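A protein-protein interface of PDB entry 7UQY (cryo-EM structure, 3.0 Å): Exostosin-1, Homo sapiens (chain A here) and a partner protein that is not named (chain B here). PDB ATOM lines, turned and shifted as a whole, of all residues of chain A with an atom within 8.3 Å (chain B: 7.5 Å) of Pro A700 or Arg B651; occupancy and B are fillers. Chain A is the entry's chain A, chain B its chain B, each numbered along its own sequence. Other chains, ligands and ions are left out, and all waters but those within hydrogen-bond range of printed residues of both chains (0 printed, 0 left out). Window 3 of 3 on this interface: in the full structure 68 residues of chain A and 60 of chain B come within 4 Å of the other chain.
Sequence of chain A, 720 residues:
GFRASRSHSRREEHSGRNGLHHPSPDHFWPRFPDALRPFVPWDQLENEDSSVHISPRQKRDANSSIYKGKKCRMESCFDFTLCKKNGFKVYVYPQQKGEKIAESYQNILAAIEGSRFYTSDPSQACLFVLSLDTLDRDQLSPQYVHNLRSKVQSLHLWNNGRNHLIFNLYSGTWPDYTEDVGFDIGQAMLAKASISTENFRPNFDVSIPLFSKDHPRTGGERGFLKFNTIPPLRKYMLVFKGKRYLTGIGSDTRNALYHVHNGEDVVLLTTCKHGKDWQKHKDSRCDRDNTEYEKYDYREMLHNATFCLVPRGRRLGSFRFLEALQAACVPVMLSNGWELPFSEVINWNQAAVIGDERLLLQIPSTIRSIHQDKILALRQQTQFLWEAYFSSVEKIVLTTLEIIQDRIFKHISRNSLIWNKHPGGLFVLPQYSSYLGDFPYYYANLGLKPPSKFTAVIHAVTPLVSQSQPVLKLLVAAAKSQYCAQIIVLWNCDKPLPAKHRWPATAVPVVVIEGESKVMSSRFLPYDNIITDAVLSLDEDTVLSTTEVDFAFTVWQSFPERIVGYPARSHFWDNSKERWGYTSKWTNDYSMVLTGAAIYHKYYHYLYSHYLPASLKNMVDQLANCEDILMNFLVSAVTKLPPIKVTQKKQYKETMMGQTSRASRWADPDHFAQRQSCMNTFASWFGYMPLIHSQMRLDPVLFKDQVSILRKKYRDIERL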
ATOM      1  N   THR A 547      18.591 -23.299   1.664  1.00  0.00           N
ATOM      2  CA  THR A 547      18.445 -23.199   0.216  1.00  0.00           C
ATOM      3  C   THR A 547      17.155 -22.488  -0.153  1.00  0.00           C
ATOM      4  O   THR A 547      17.101 -21.767  -1.157  1.00  0.00           O
ATOM      5  CB  THR A 547      18.480 -24.590  -0.419  1.00  0.00           C
ATOM      6  OG1 THR A 547      17.245 -25.267  -0.157  1.00  0.00           O
ATOM      7  CG2 THR A 547      19.631 -25.406   0.151  1.00  0.00           C
ATOM      8  N   GLU A 548      16.110 -22.680   0.651  1.00  0.00           N
ATOM      9  CA  GLU A 548      14.851 -21.983   0.426  1.00  0.00           C
ATOM     10  C   GLU A 548      15.021 -20.477   0.609  1.00  0.00           C
ATOM     11  O   GLU A 548      14.503 -19.683  -0.187  1.00  0.00           O
ATOM     12  CB  GLU A 548      13.797 -22.561   1.372  1.00  0.00           C
ATOM     13  CG  GLU A 548      12.409 -22.014   1.219  1.00  0.00           C
ATOM     14  CD  GLU A 548      11.417 -22.679   2.155  1.00  0.00           C
ATOM     15  OE1 GLU A 548      11.835 -23.558   2.938  1.00  0.00           O
ATOM     16  OE2 GLU A 548      10.222 -22.321   2.108  1.00  0.00           O
ATOM     17  N   PHE A 551      16.914 -19.200  -2.488  1.00  0.00           N
ATOM     18  CA  PHE A 551      16.029 -19.065  -3.639  1.00  0.00           C
ATOM     19  C   PHE A 551      15.121 -17.853  -3.497  1.00  0.00           C
ATOM     20  O   PHE A 551      14.906 -17.114  -4.465  1.00  0.00           O
ATOM     21  CB  PHE A 551      15.194 -20.331  -3.823  1.00  0.00           C
ATOM     22  CG  PHE A 551      14.179 -20.223  -4.923  1.00  0.00           C
ATOM     23  CD1 PHE A 551      14.578 -20.104  -6.243  1.00  0.00           C
ATOM     24  CD2 PHE A 551      12.824 -20.228  -4.636  1.00  0.00           C
ATOM     25  CE1 PHE A 551      13.646 -19.998  -7.258  1.00  0.00           C
ATOM     26  CE2 PHE A 551      11.888 -20.122  -5.646  1.00  0.00           C
ATOM     27  CZ  PHE A 551      12.299 -20.006  -6.958  1.00  0.00           C
ATOM     28  N   ALA A 552      14.577 -17.631  -2.298  1.00  0.00           N
ATOM     29  CA  ALA A 552      13.724 -16.468  -2.090  1.00  0.00           C
ATOM     30  C   ALA A 552      14.488 -15.176  -2.343  1.00  0.00           C
ATOM     31  O   ALA A 552      13.971 -14.255  -2.986  1.00  0.00           O
ATOM     32  CB  ALA A 552      13.147 -16.486  -0.675  1.00  0.00           C
ATOM     33  N   THR A 554      17.196 -14.762  -4.240  1.00  0.00           N
ATOM     34  CA  THR A 554      17.506 -14.631  -5.661  1.00  0.00           C
ATOM     35  C   THR A 554      16.283 -14.188  -6.453  1.00  0.00           C
ATOM     36  O   THR A 554      16.401 -13.391  -7.391  1.00  0.00           O
ATOM     37  CB  THR A 554      18.060 -15.943  -6.212  1.00  0.00           C
ATOM     38  OG1 THR A 554      17.105 -16.993  -6.015  1.00  0.00           O
ATOM     39  CG2 THR A 554      19.378 -16.300  -5.539  1.00  0.00           C
ATOM     40  N   VAL A 555      15.101 -14.699  -6.098  1.00  0.00           N
ATOM     41  CA  VAL A 555      13.878 -14.239  -6.752  1.00  0.00           C
ATOM     42  C   VAL A 555      13.631 -12.768  -6.449  1.00  0.00           C
ATOM     43  O   VAL A 555      13.273 -11.987  -7.339  1.00  0.00           O
ATOM     44  CB  VAL A 555      12.679 -15.110  -6.336  1.00  0.00           C
ATOM     45  CG1 VAL A 555      11.397 -14.563  -6.936  1.00  0.00           C
ATOM     46  CG2 VAL A 555      12.891 -16.539  -6.791  1.00  0.00           C
ATOM     47  N   TYR A 566       6.665 -16.986   0.932  1.00  0.00           N
ATOM     48  CA  TYR A 566       6.039 -18.292   0.775  1.00  0.00           C
ATOM     49  C   TYR A 566       4.575 -18.318   1.219  1.00  0.00           C
ATOM     50  O   TYR A 566       3.719 -18.756   0.440  1.00  0.00           O
ATOM     51  CB  TYR A 566       6.883 -19.342   1.505  1.00  0.00           C
ATOM     52  CG  TYR A 566       8.280 -19.424   0.927  1.00  0.00           C
ATOM     53  CD1 TYR A 566       9.253 -18.497   1.278  1.00  0.00           C
ATOM     54  CD2 TYR A 566       8.613 -20.399   0.000  1.00  0.00           C
ATOM     55  CE1 TYR A 566      10.518 -18.550   0.737  1.00  0.00           C
ATOM     56  CE2 TYR A 566       9.877 -20.461  -0.547  1.00  0.00           C
ATOM     57  CZ  TYR A 566      10.825 -19.531  -0.176  1.00  0.00           C
ATOM     58  OH  TYR A 566      12.090 -19.589  -0.715  1.00  0.00           O
ATOM     59  N   LYS A 645       4.635 -14.970  -4.924  1.00  0.00           N
ATOM     60  CA  LYS A 645       4.740 -16.144  -4.074  1.00  0.00           C
ATOM     61  C   LYS A 645       5.691 -17.152  -4.703  1.00  0.00           C
ATOM     62  O   LYS A 645       5.648 -17.393  -5.913  1.00  0.00           O
ATOM     63  CB  LYS A 645       3.370 -16.789  -3.858  1.00  0.00           C
ATOM     64  CG  LYS A 645       3.428 -18.124  -3.138  1.00  0.00           C
ATOM     65  CD  LYS A 645       2.077 -18.810  -3.122  1.00  0.00           C
ATOM     66  CE  LYS A 645       2.204 -20.256  -2.675  1.00  0.00           C
ATOM     67  NZ  LYS A 645       2.672 -20.361  -1.266  1.00  0.00           N
ATOM     68  N   VAL A 646       6.552 -17.739  -3.872  1.00  0.00           N
ATOM     69  CA  VAL A 646       7.517 -18.730  -4.316  1.00  0.00           C
ATOM     70  C   VAL A 646       7.339 -19.994  -3.486  1.00  0.00           C
ATOM     71  O   VAL A 646       6.822 -19.963  -2.367  1.00  0.00           O
ATOM     72  CB  VAL A 646       8.965 -18.211  -4.215  1.00  0.00           C
ATOM     73  CG1 VAL A 646       9.154 -17.003  -5.116  1.00  0.00           C
ATOM     74  CG2 VAL A 646       9.293 -17.844  -2.782  1.00  0.00           C
ATOM     75  N   THR A 647       7.754 -21.121  -4.062  1.00  0.00           N
ATOM     76  CA  THR A 647       7.740 -22.403  -3.374  1.00  0.00           C
ATOM     77  C   THR A 647       9.010 -23.165  -3.723  1.00  0.00           C
ATOM     78  O   THR A 647       9.787 -22.757  -4.592  1.00  0.00           O
ATOM     79  CB  THR A 647       6.508 -23.246  -3.736  1.00  0.00           C
ATOM     80  OG1 THR A 647       5.319 -22.548  -3.353  1.00  0.00           O
ATOM     81  CG2 THR A 647       6.547 -24.596  -3.041  1.00  0.00           C
ATOM     82  N   GLN A 648       9.212 -24.283  -3.029  1.00  0.00           N
ATOM     83  CA  GLN A 648      10.351 -25.172  -3.260  1.00  0.00           C
ATOM     84  C   GLN A 648      11.685 -24.441  -3.127  1.00  0.00           C
ATOM     85  O   GLN A 648      12.676 -25.012  -2.673  1.00  0.00           O
ATOM     86  CB  GLN A 648      10.246 -25.827  -4.641  1.00  0.00           C
ATOM     87  CG  GLN A 648      11.195 -26.996  -4.852  1.00  0.00           C
ATOM     88  CD  GLN A 648      10.988 -27.680  -6.190  1.00  0.00           C
ATOM     89  OE1 GLN A 648      10.115 -27.295  -6.969  1.00  0.00           O
ATOM     90  NE2 GLN A 648      11.792 -28.701  -6.463  1.00  0.00           N
ATOM     91  N   MET A 696       0.137 -16.690 -10.325  1.00  0.00           N
ATOM     92  CA  MET A 696       1.325 -17.464 -10.646  1.00  0.00           C
ATOM     93  C   MET A 696       2.043 -17.891  -9.368  1.00  0.00           C
ATOM     94  O   MET A 696       1.664 -17.521  -8.256  1.00  0.00           O
ATOM     95  CB  MET A 696       2.268 -16.654 -11.537  1.00  0.00           C
ATOM     96  CG  MET A 696       3.176 -15.731 -10.753  1.00  0.00           C
ATOM     97  SD  MET A 696       3.947 -14.458 -11.757  1.00  0.00           S
ATOM     98  CE  MET A 696       5.280 -13.962 -10.670  1.00  0.00           C
ATOM     99  N   ARG A 697       3.097 -18.689  -9.542  1.00  0.00           N
ATOM    100  CA  ARG A 697       3.900 -19.155  -8.411  1.00  0.00           C
ATOM    101  C   ARG A 697       5.293 -19.483  -8.941  1.00  0.00           C
ATOM    102  O   ARG A 697       5.476 -20.495  -9.624  1.00  0.00           O
ATOM    103  CB  ARG A 697       3.250 -20.357  -7.740  1.00  0.00           C
ATOM    104  CG  ARG A 697       4.150 -21.111  -6.784  1.00  0.00           C
ATOM    105  CD  ARG A 697       3.530 -22.439  -6.383  1.00  0.00           C
ATOM    106  NE  ARG A 697       3.434 -23.371  -7.499  1.00  0.00           N
ATOM    107  CZ  ARG A 697       3.061 -24.637  -7.384  1.00  0.00           C
ATOM    108  NH1 ARG A 697       2.749 -25.162  -6.210  1.00  0.00           N
ATOM    109  NH2 ARG A 697       2.999 -25.398  -8.473  1.00  0.00           N
ATOM    110  N   LEU A 698       6.262 -18.623  -8.635  1.00  0.00           N
ATOM    111  CA  LEU A 698       7.617 -18.818  -9.133  1.00  0.00           C
ATOM    112  C   LEU A 698       8.303 -19.962  -8.396  1.00  0.00           C
ATOM    113  O   LEU A 698       8.305 -20.010  -7.163  1.00  0.00           O
ATOM    114  CB  LEU A 698       8.426 -17.532  -8.990  1.00  0.00           C
ATOM    115  CG  LEU A 698       7.982 -16.366  -9.873  1.00  0.00           C
ATOM    116  CD1 LEU A 698       9.070 -15.315  -9.955  1.00  0.00           C
ATOM    117  CD2 LEU A 698       7.604 -16.854 -11.261  1.00  0.00           C
ATOM    118  N   ASP A 699       8.890 -20.881  -9.157  1.00  0.00           N
ATOM    119  CA  ASP A 699       9.583 -22.039  -8.622  1.00  0.00           C
ATOM    120  C   ASP A 699      10.939 -22.193  -9.294  1.00  0.00           C
ATOM    121  O   ASP A 699      11.134 -21.721 -10.418  1.00  0.00           O
ATOM    122  CB  ASP A 699       8.759 -23.319  -8.824  1.00  0.00           C
ATOM    123  CG  ASP A 699       7.517 -23.350  -7.962  1.00  0.00           C
ATOM    124  OD1 ASP A 699       7.537 -22.738  -6.874  1.00  0.00           O
ATOM    125  OD2 ASP A 699       6.525 -23.990  -8.364  1.00  0.00           O
ATOM    126  N   PRO A 700      11.896 -22.837  -8.628  1.00  0.00           N
ATOM    127  CA  PRO A 700      13.205 -23.045  -9.253  1.00  0.00           C
ATOM    128  C   PRO A 700      13.105 -23.957 -10.463  1.00  0.00           C
ATOM    129  O   PRO A 700      12.245 -24.836 -10.542  1.00  0.00           O
ATOM    130  CB  PRO A 700      14.035 -23.690  -8.137  1.00  0.00           C
ATOM    131  CG  PRO A 700      13.032 -24.306  -7.227  1.00  0.00           C
ATOM    132  CD  PRO A 700      11.837 -23.407  -7.270  1.00  0.00           C
ATOM    133  N   VAL A 701      14.004 -23.734 -11.415  1.00  0.00           N
ATOM    134  CA  VAL A 701      14.026 -24.524 -12.636  1.00  0.00           C
ATOM    135  C   VAL A 701      14.918 -25.747 -12.461  1.00  0.00           C
ATOM    136  O   VAL A 701      14.652 -26.608 -11.622  1.00  0.00           O
ATOM    137  CB  VAL A 701      14.491 -23.686 -13.832  1.00  0.00           C
ATOM    138  CG1 VAL A 701      14.603 -24.556 -15.068  1.00  0.00           C
ATOM    139  CG2 VAL A 701      13.538 -22.528 -14.071  1.00  0.00           C
ATOM    140  N   PHE B 507      -2.867 -20.834 -19.369  1.00  0.00           N
ATOM    141  CA  PHE B 507      -2.065 -20.421 -18.223  1.00  0.00           C
ATOM    142  C   PHE B 507      -0.935 -19.490 -18.641  1.00  0.00           C
ATOM    143  O   PHE B 507      -0.588 -18.560 -17.907  1.00  0.00           O
ATOM    144  CB  PHE B 507      -1.504 -21.638 -17.495  1.00  0.00           C
ATOM    145  CG  PHE B 507      -0.701 -21.287 -16.281  1.00  0.00           C
ATOM    146  CD1 PHE B 507      -1.328 -20.890 -15.112  1.00  0.00           C
ATOM    147  CD2 PHE B 507       0.681 -21.329 -16.314  1.00  0.00           C
ATOM    148  CE1 PHE B 507      -0.591 -20.557 -13.995  1.00  0.00           C
ATOM    149  CE2 PHE B 507       1.421 -20.995 -15.201  1.00  0.00           C
ATOM    150  CZ  PHE B 507       0.784 -20.608 -14.040  1.00  0.00           C
ATOM    151  N   THR B 543      19.506 -27.535 -17.851  1.00  0.00           N
ATOM    152  CA  THR B 543      18.814 -26.287 -17.535  1.00  0.00           C
ATOM    153  C   THR B 543      18.790 -26.115 -16.020  1.00  0.00           C
ATOM    154  O   THR B 543      17.914 -26.656 -15.338  1.00  0.00           O
ATOM    155  CB  THR B 543      17.406 -26.275 -18.118  1.00  0.00           C
ATOM    156  OG1 THR B 543      17.473 -26.522 -19.528  1.00  0.00           O
ATOM    157  CG2 THR B 543      16.757 -24.921 -17.894  1.00  0.00           C
ATOM    158  N   ASN B 544      19.763 -25.365 -15.499  1.00  0.00           N
ATOM    159  CA  ASN B 544      19.732 -24.885 -14.127  1.00  0.00           C
ATOM    160  C   ASN B 544      19.378 -23.411 -14.029  1.00  0.00           C
ATOM    161  O   ASN B 544      18.863 -22.981 -12.992  1.00  0.00           O
ATOM    162  CB  ASN B 544      21.087 -25.122 -13.442  1.00  0.00           C
ATOM    163  CG  ASN B 544      21.003 -25.018 -11.931  1.00  0.00           C
ATOM    164  OD1 ASN B 544      19.954 -25.269 -11.338  1.00  0.00           O
ATOM    165  ND2 ASN B 544      22.110 -24.645 -11.302  1.00  0.00           N
ATOM    166  N   VAL B 546      17.823 -20.011 -16.721  1.00  0.00           N
ATOM    167  CA  VAL B 546      17.188 -19.689 -17.992  1.00  0.00           C
ATOM    168  C   VAL B 546      17.501 -18.241 -18.330  1.00  0.00           C
ATOM    169  O   VAL B 546      17.300 -17.347 -17.502  1.00  0.00           O
ATOM    170  CB  VAL B 546      15.667 -19.922 -17.952  1.00  0.00           C
ATOM    171  CG1 VAL B 546      14.991 -19.231 -19.124  1.00  0.00           C
ATOM    172  CG2 VAL B 546      15.359 -21.409 -17.955  1.00  0.00           C
ATOM    173  N   VAL B 599      13.242 -13.000 -18.161  1.00  0.00           N
ATOM    174  CA  VAL B 599      12.301 -13.732 -18.994  1.00  0.00           C
ATOM    175  C   VAL B 599      11.605 -14.776 -18.132  1.00  0.00           C
ATOM    176  O   VAL B 599      12.186 -15.309 -17.181  1.00  0.00           O
ATOM    177  CB  VAL B 599      13.010 -14.384 -20.202  1.00  0.00           C
ATOM    178  CG1 VAL B 599      13.994 -15.452 -19.742  1.00  0.00           C
ATOM    179  CG2 VAL B 599      12.002 -14.949 -21.167  1.00  0.00           C
ATOM    180  N   ILE B 600      10.346 -15.057 -18.457  1.00  0.00           N
ATOM    181  CA  ILE B 600       9.512 -15.955 -17.667  1.00  0.00           C
ATOM    182  C   ILE B 600       9.230 -17.208 -18.480  1.00  0.00           C
ATOM    183  O   ILE B 600       8.645 -17.136 -19.568  1.00  0.00           O
ATOM    184  CB  ILE B 600       8.205 -15.278 -17.231  1.00  0.00           C
ATOM    185  CG1 ILE B 600       8.503 -14.031 -16.399  1.00  0.00           C
ATOM    186  CG2 ILE B 600       7.344 -16.246 -16.440  1.00  0.00           C
ATOM    187  CD1 ILE B 600       9.268 -14.315 -15.126  1.00  0.00           C
ATOM    188  N   LYS B 601       9.643 -18.355 -17.950  1.00  0.00           N
ATOM    189  CA  LYS B 601       9.275 -19.652 -18.498  1.00  0.00           C
ATOM    190  C   LYS B 601       8.105 -20.203 -17.694  1.00  0.00           C
ATOM    191  O   LYS B 601       8.149 -20.221 -16.460  1.00  0.00           O
ATOM    192  CB  LYS B 601      10.461 -20.614 -18.452  1.00  0.00           C
ATOM    193  CG  LYS B 601      10.233 -21.922 -19.181  1.00  0.00           C
ATOM    194  CD  LYS B 601      11.137 -23.015 -18.637  1.00  0.00           C
ATOM    195  CE  LYS B 601      11.079 -24.259 -19.505  1.00  0.00           C
ATOM    196  NZ  LYS B 601       9.696 -24.529 -19.984  1.00  0.00           N
ATOM    197  N   VAL B 602       7.059 -20.648 -18.389  1.00  0.00           N
ATOM    198  CA  VAL B 602       5.803 -20.970 -17.722  1.00  0.00           C
ATOM    199  C   VAL B 602       5.442 -22.442 -17.851  1.00  0.00           C
ATOM    200  O   VAL B 602       4.259 -22.800 -17.865  1.00  0.00           O
ATOM    201  CB  VAL B 602       4.663 -20.083 -18.253  1.00  0.00           C
ATOM    202  CG1 VAL B 602       4.959 -18.633 -17.956  1.00  0.00           C
ATOM    203  CG2 VAL B 602       4.491 -20.282 -19.752  1.00  0.00           C
ATOM    204  N   THR B 603       6.444 -23.308 -17.925  1.00  0.00           N
ATOM    205  CA  THR B 603       6.160 -24.736 -17.988  1.00  0.00           C
ATOM    206  C   THR B 603       7.353 -25.549 -17.503  1.00  0.00           C
ATOM    207  O   THR B 603       8.483 -25.324 -17.950  1.00  0.00           O
ATOM    208  CB  THR B 603       5.783 -25.151 -19.412  1.00  0.00           C
ATOM    209  OG1 THR B 603       4.550 -24.523 -19.782  1.00  0.00           O
ATOM    210  CG2 THR B 603       5.616 -26.659 -19.506  1.00  0.00           C
ATOM    211  N   PRO B 604       7.143 -26.503 -16.590  1.00  0.00           N
ATOM    212  CA  PRO B 604       8.214 -27.401 -16.140  1.00  0.00           C
ATOM    213  C   PRO B 604       8.467 -28.566 -17.098  1.00  0.00           C
ATOM    214  O   PRO B 604       8.561 -29.724 -16.687  1.00  0.00           O
ATOM    215  CB  PRO B 604       7.697 -27.887 -14.783  1.00  0.00           C
ATOM    216  CG  PRO B 604       6.218 -27.873 -14.933  1.00  0.00           C
ATOM    217  CD  PRO B 604       5.890 -26.719 -15.846  1.00  0.00           C
ATOM    218  N   ARG B 605       8.577 -28.254 -18.388  1.00  0.00           N
ATOM    219  CA  ARG B 605       8.820 -29.255 -19.414  1.00  0.00           C
ATOM    220  C   ARG B 605       9.791 -28.687 -20.439  1.00  0.00           C
ATOM    221  O   ARG B 605       9.836 -27.476 -20.667  1.00  0.00           O
ATOM    222  CB  ARG B 605       7.512 -29.691 -20.090  1.00  0.00           C
ATOM    223  CG  ARG B 605       7.591 -31.017 -20.830  1.00  0.00           C
ATOM    224  CD  ARG B 605       6.505 -31.116 -21.888  1.00  0.00           C
ATOM    225  NE  ARG B 605       5.200 -30.726 -21.367  1.00  0.00           N
ATOM    226  CZ  ARG B 605       4.285 -31.578 -20.924  1.00  0.00           C
ATOM    227  NH1 ARG B 605       4.497 -32.883 -20.925  1.00  0.00           N
ATOM    228  NH2 ARG B 605       3.128 -31.106 -20.470  1.00  0.00           N
ATOM    229  N   LYS B 606      10.568 -29.575 -21.055  1.00  0.00           N
ATOM    230  CA  LYS B 606      11.600 -29.187 -22.008  1.00  0.00           C
ATOM    231  C   LYS B 606      11.272 -29.590 -23.437  1.00  0.00           C
ATOM    232  O   LYS B 606      11.472 -28.798 -24.364  1.00  0.00           O
ATOM    233  CB  LYS B 606      12.949 -29.795 -21.596  1.00  0.00           C
ATOM    234  CG  LYS B 606      13.416 -29.378 -20.213  1.00  0.00           C
ATOM    235  CD  LYS B 606      14.747 -30.022 -19.862  1.00  0.00           C
ATOM    236  CE  LYS B 606      15.171 -29.669 -18.447  1.00  0.00           C
ATOM    237  NZ  LYS B 606      16.490 -30.263 -18.099  1.00  0.00           N
ATOM    238  N   VAL B 648      18.220 -15.961 -14.840  1.00  0.00           N
ATOM    239  CA  VAL B 648      17.300 -16.192 -13.734  1.00  0.00           C
ATOM    240  C   VAL B 648      16.942 -17.670 -13.701  1.00  0.00           C
ATOM    241  O   VAL B 648      17.040 -18.380 -14.703  1.00  0.00           O
ATOM    242  CB  VAL B 648      16.023 -15.333 -13.838  1.00  0.00           C
ATOM    243  CG1 VAL B 648      16.359 -13.863 -13.664  1.00  0.00           C
ATOM    244  CG2 VAL B 648      15.335 -15.571 -15.170  1.00  0.00           C
ATOM    245  N   GLU B 649      16.520 -18.131 -12.523  1.00  0.00           N
ATOM    246  CA  GLU B 649      16.206 -19.540 -12.312  1.00  0.00           C
ATOM    247  C   GLU B 649      14.794 -19.751 -11.777  1.00  0.00           C
ATOM    248  O   GLU B 649      14.510 -20.793 -11.178  1.00  0.00           O
ATOM    249  CB  GLU B 649      17.234 -20.177 -11.375  1.00  0.00           C
ATOM    250  CG  GLU B 649      17.174 -19.689  -9.938  1.00  0.00           C
ATOM    251  CD  GLU B 649      17.965 -18.416  -9.719  1.00  0.00           C
ATOM    252  OE1 GLU B 649      18.311 -17.744 -10.714  1.00  0.00           O
ATOM    253  OE2 GLU B 649      18.247 -18.088  -8.548  1.00  0.00           O
ATOM    254  N   HIS B 650      13.895 -18.795 -11.993  1.00  0.00           N
ATOM    255  CA  HIS B 650      12.523 -18.893 -11.518  1.00  0.00           C
ATOM    256  C   HIS B 650      11.587 -19.124 -12.696  1.00  0.00           C
ATOM    257  O   HIS B 650      11.667 -18.418 -13.707  1.00  0.00           O
ATOM    258  CB  HIS B 650      12.114 -17.634 -10.750  1.00  0.00           C
ATOM    259  CG  HIS B 650      12.463 -16.357 -11.446  1.00  0.00           C
ATOM    260  ND1 HIS B 650      11.685 -15.821 -12.450  1.00  0.00           N
ATOM    261  CD2 HIS B 650      13.499 -15.503 -11.277  1.00  0.00           C
ATOM    262  CE1 HIS B 650      12.230 -14.695 -12.872  1.00  0.00           C
ATOM    263  NE2 HIS B 650      13.330 -14.479 -12.176  1.00  0.00           N
ATOM    264  N   ARG B 651      10.708 -20.114 -12.561  1.00  0.00           N
ATOM    265  CA  ARG B 651       9.689 -20.423 -13.551  1.00  0.00           C
ATOM    266  C   ARG B 651       8.315 -20.385 -12.894  1.00  0.00           C
ATOM    267  O   ARG B 651       8.174 -20.605 -11.688  1.00  0.00           O
ATOM    268  CB  ARG B 651       9.922 -21.797 -14.190  1.00  0.00           C
ATOM    269  CG  ARG B 651       9.727 -22.962 -13.234  1.00  0.00           C
ATOM    270  CD  ARG B 651       9.052 -24.137 -13.920  1.00  0.00           C
ATOM    271  NE  ARG B 651       9.154 -25.359 -13.133  1.00  0.00           N
ATOM    272  CZ  ARG B 651      10.211 -26.159 -13.123  1.00  0.00           C
ATOM    273  NH1 ARG B 651      11.277 -25.905 -13.865  1.00  0.00           N
ATOM    274  NH2 ARG B 651      10.198 -27.244 -12.353  1.00  0.00           N
ATOM    275  N   ALA B 652       7.297 -20.114 -13.704  1.00  0.00           N
ATOM    276  CA  ALA B 652       5.930 -19.965 -13.222  1.00  0.00           C
ATOM    277  C   ALA B 652       5.116 -21.204 -13.571  1.00  0.00           C
ATOM    278  O   ALA B 652       5.116 -21.650 -14.722  1.00  0.00           O
ATOM    279  CB  ALA B 652       5.277 -18.719 -13.821  1.00  0.00           C
ATOM    280  N   ASP B 653       4.430 -21.756 -12.579  1.00  0.00           N
ATOM    281  CA  ASP B 653       3.563 -22.908 -12.764  1.00  0.00           C
ATOM    282  C   ASP B 653       2.271 -22.675 -11.997  1.00  0.00           C
ATOM    283  O   ASP B 653       2.206 -21.789 -11.139  1.00  0.00           O
ATOM    284  CB  ASP B 653       4.236 -24.210 -12.303  1.00  0.00           C
ATOM    285  CG  ASP B 653       4.660 -24.172 -10.851  1.00  0.00           C
ATOM    286  OD1 ASP B 653       4.635 -23.082 -10.244  1.00  0.00           O
ATOM    287  OD2 ASP B 653       5.015 -25.242 -10.314  1.00  0.00           O
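Among the printed residues, pairs that only touch across the chains: Arg A697 with Ala B652 (3.7 Å), Leu A698 with His B650 (3.6 Å), Leu A698 with Arg B651 (3.2 Å), Leu A698 with Ala B652 (3.9 Å), Asp A699 with Glu B649 (3.6 Å), Asp A699 with His B650 (3.3 Å), Pro A700 with Glu B649 (3.2 Å), Pro A700 with Arg B651 (3.5 Å), Val A701 with Thr B543 (3.6 Å) and Val A701 with Arg B651 (3.3 Å).
The side-chain carboxylate (OD2) of Asp B653 sits close to the side-chain carboxylate (OD2) of Asp A699, at 2.8 Å. The side-chain hydroxyl (OG1) of Thr A554 lies within hydrogen-bond range of the side-chain carboxylate (OE2) of Glu B649 (3.0 Å). The backbone NH of Val A701 is in hydrogen-bond range of the backbone carbonyl oxygen of Glu B649, at 3.0 Å. The backbone NH (N) of Asp A699 is in hydrogen-bond range of the backbone carbonyl oxygen (O) of Arg B651, 2.6 Å away. O of Arg A697 sits close to O of Arg B651 (3.4 Å). The side-chain carboxylate (OD2) of Asp B653 is in salt-bridge range of the guanidinium group (NH2) of Arg A697 (2.7 Å).
The backbone carbonyl oxygen (O) of Lys A645 sits at hydrogen-bond distance from the backbone NH (N) of Leu A698, at 3.0 Å. O of Lys B601 lies within hydrogen-bond range of N of Ala B652. The guanidinium group of Arg A697 is in salt-bridge range of the side-chain carboxylate of Asp A699 (3.3 Å). The backbone NH (N) of Thr A647 lies within hydrogen-bond range of the backbone carbonyl oxygen (O) of Leu A698 (3.3 Å). OD1 of Asp A699 lies within hydrogen-bond range of N of Thr A647 (3.3 Å). The backbone carbonyl oxygen (O) of Phe A551 is in hydrogen-bond range of the side-chain hydroxyl (OG1) of Thr A554, 2.7 Å away.
Hydrophobic or aromatic side chains of chain A within 4 Å of the printed part of chain B: Leu A698 and Val A701. Of the 18 printed residues of chain B, 6 touch a printed residue of chain A. Hydrophobic or aromatic side chains of chain B within 4 Å of the printed part of chain A: His B650 and Ala B652. Among the printed residues, 16 pairs touch across the chains. Among the printed residues, Asp or Glu carboxylates within 4 Å of a Lys or Arg side-chain nitrogen of the other chain: Arg A697 with Asp B653.
Of the printed residues of chain B, Arg A697 touches Arg B651, Ala B652 and Asp B653. Of the printed residues of chain B, Asp A699 touches Glu B649, His B650, Arg B651 and Asp B653. Printed residues of chain B within 4 Å of Val A701: Thr B543, Glu B649 and Arg B651. Of the printed residues of chain A, Thr B543 touches Val A701 (3.6 Å). Of the printed residues of chain A, Glu B649 touches Thr A554, Asp A699, Pro A700 and Val A701. Printed residues of chain A within 4 Å of Arg B651: Arg A697, Leu A698, Asp A699, Pro A700 and Val A701. Ala B652 touches two residues of chain A. The nearest residue of chain B that does not touch Pro A700 is His B650 (4.8 Å). The nearest residue of chain A that does not touch Arg B651 is Gln A648 (5.4 Å).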
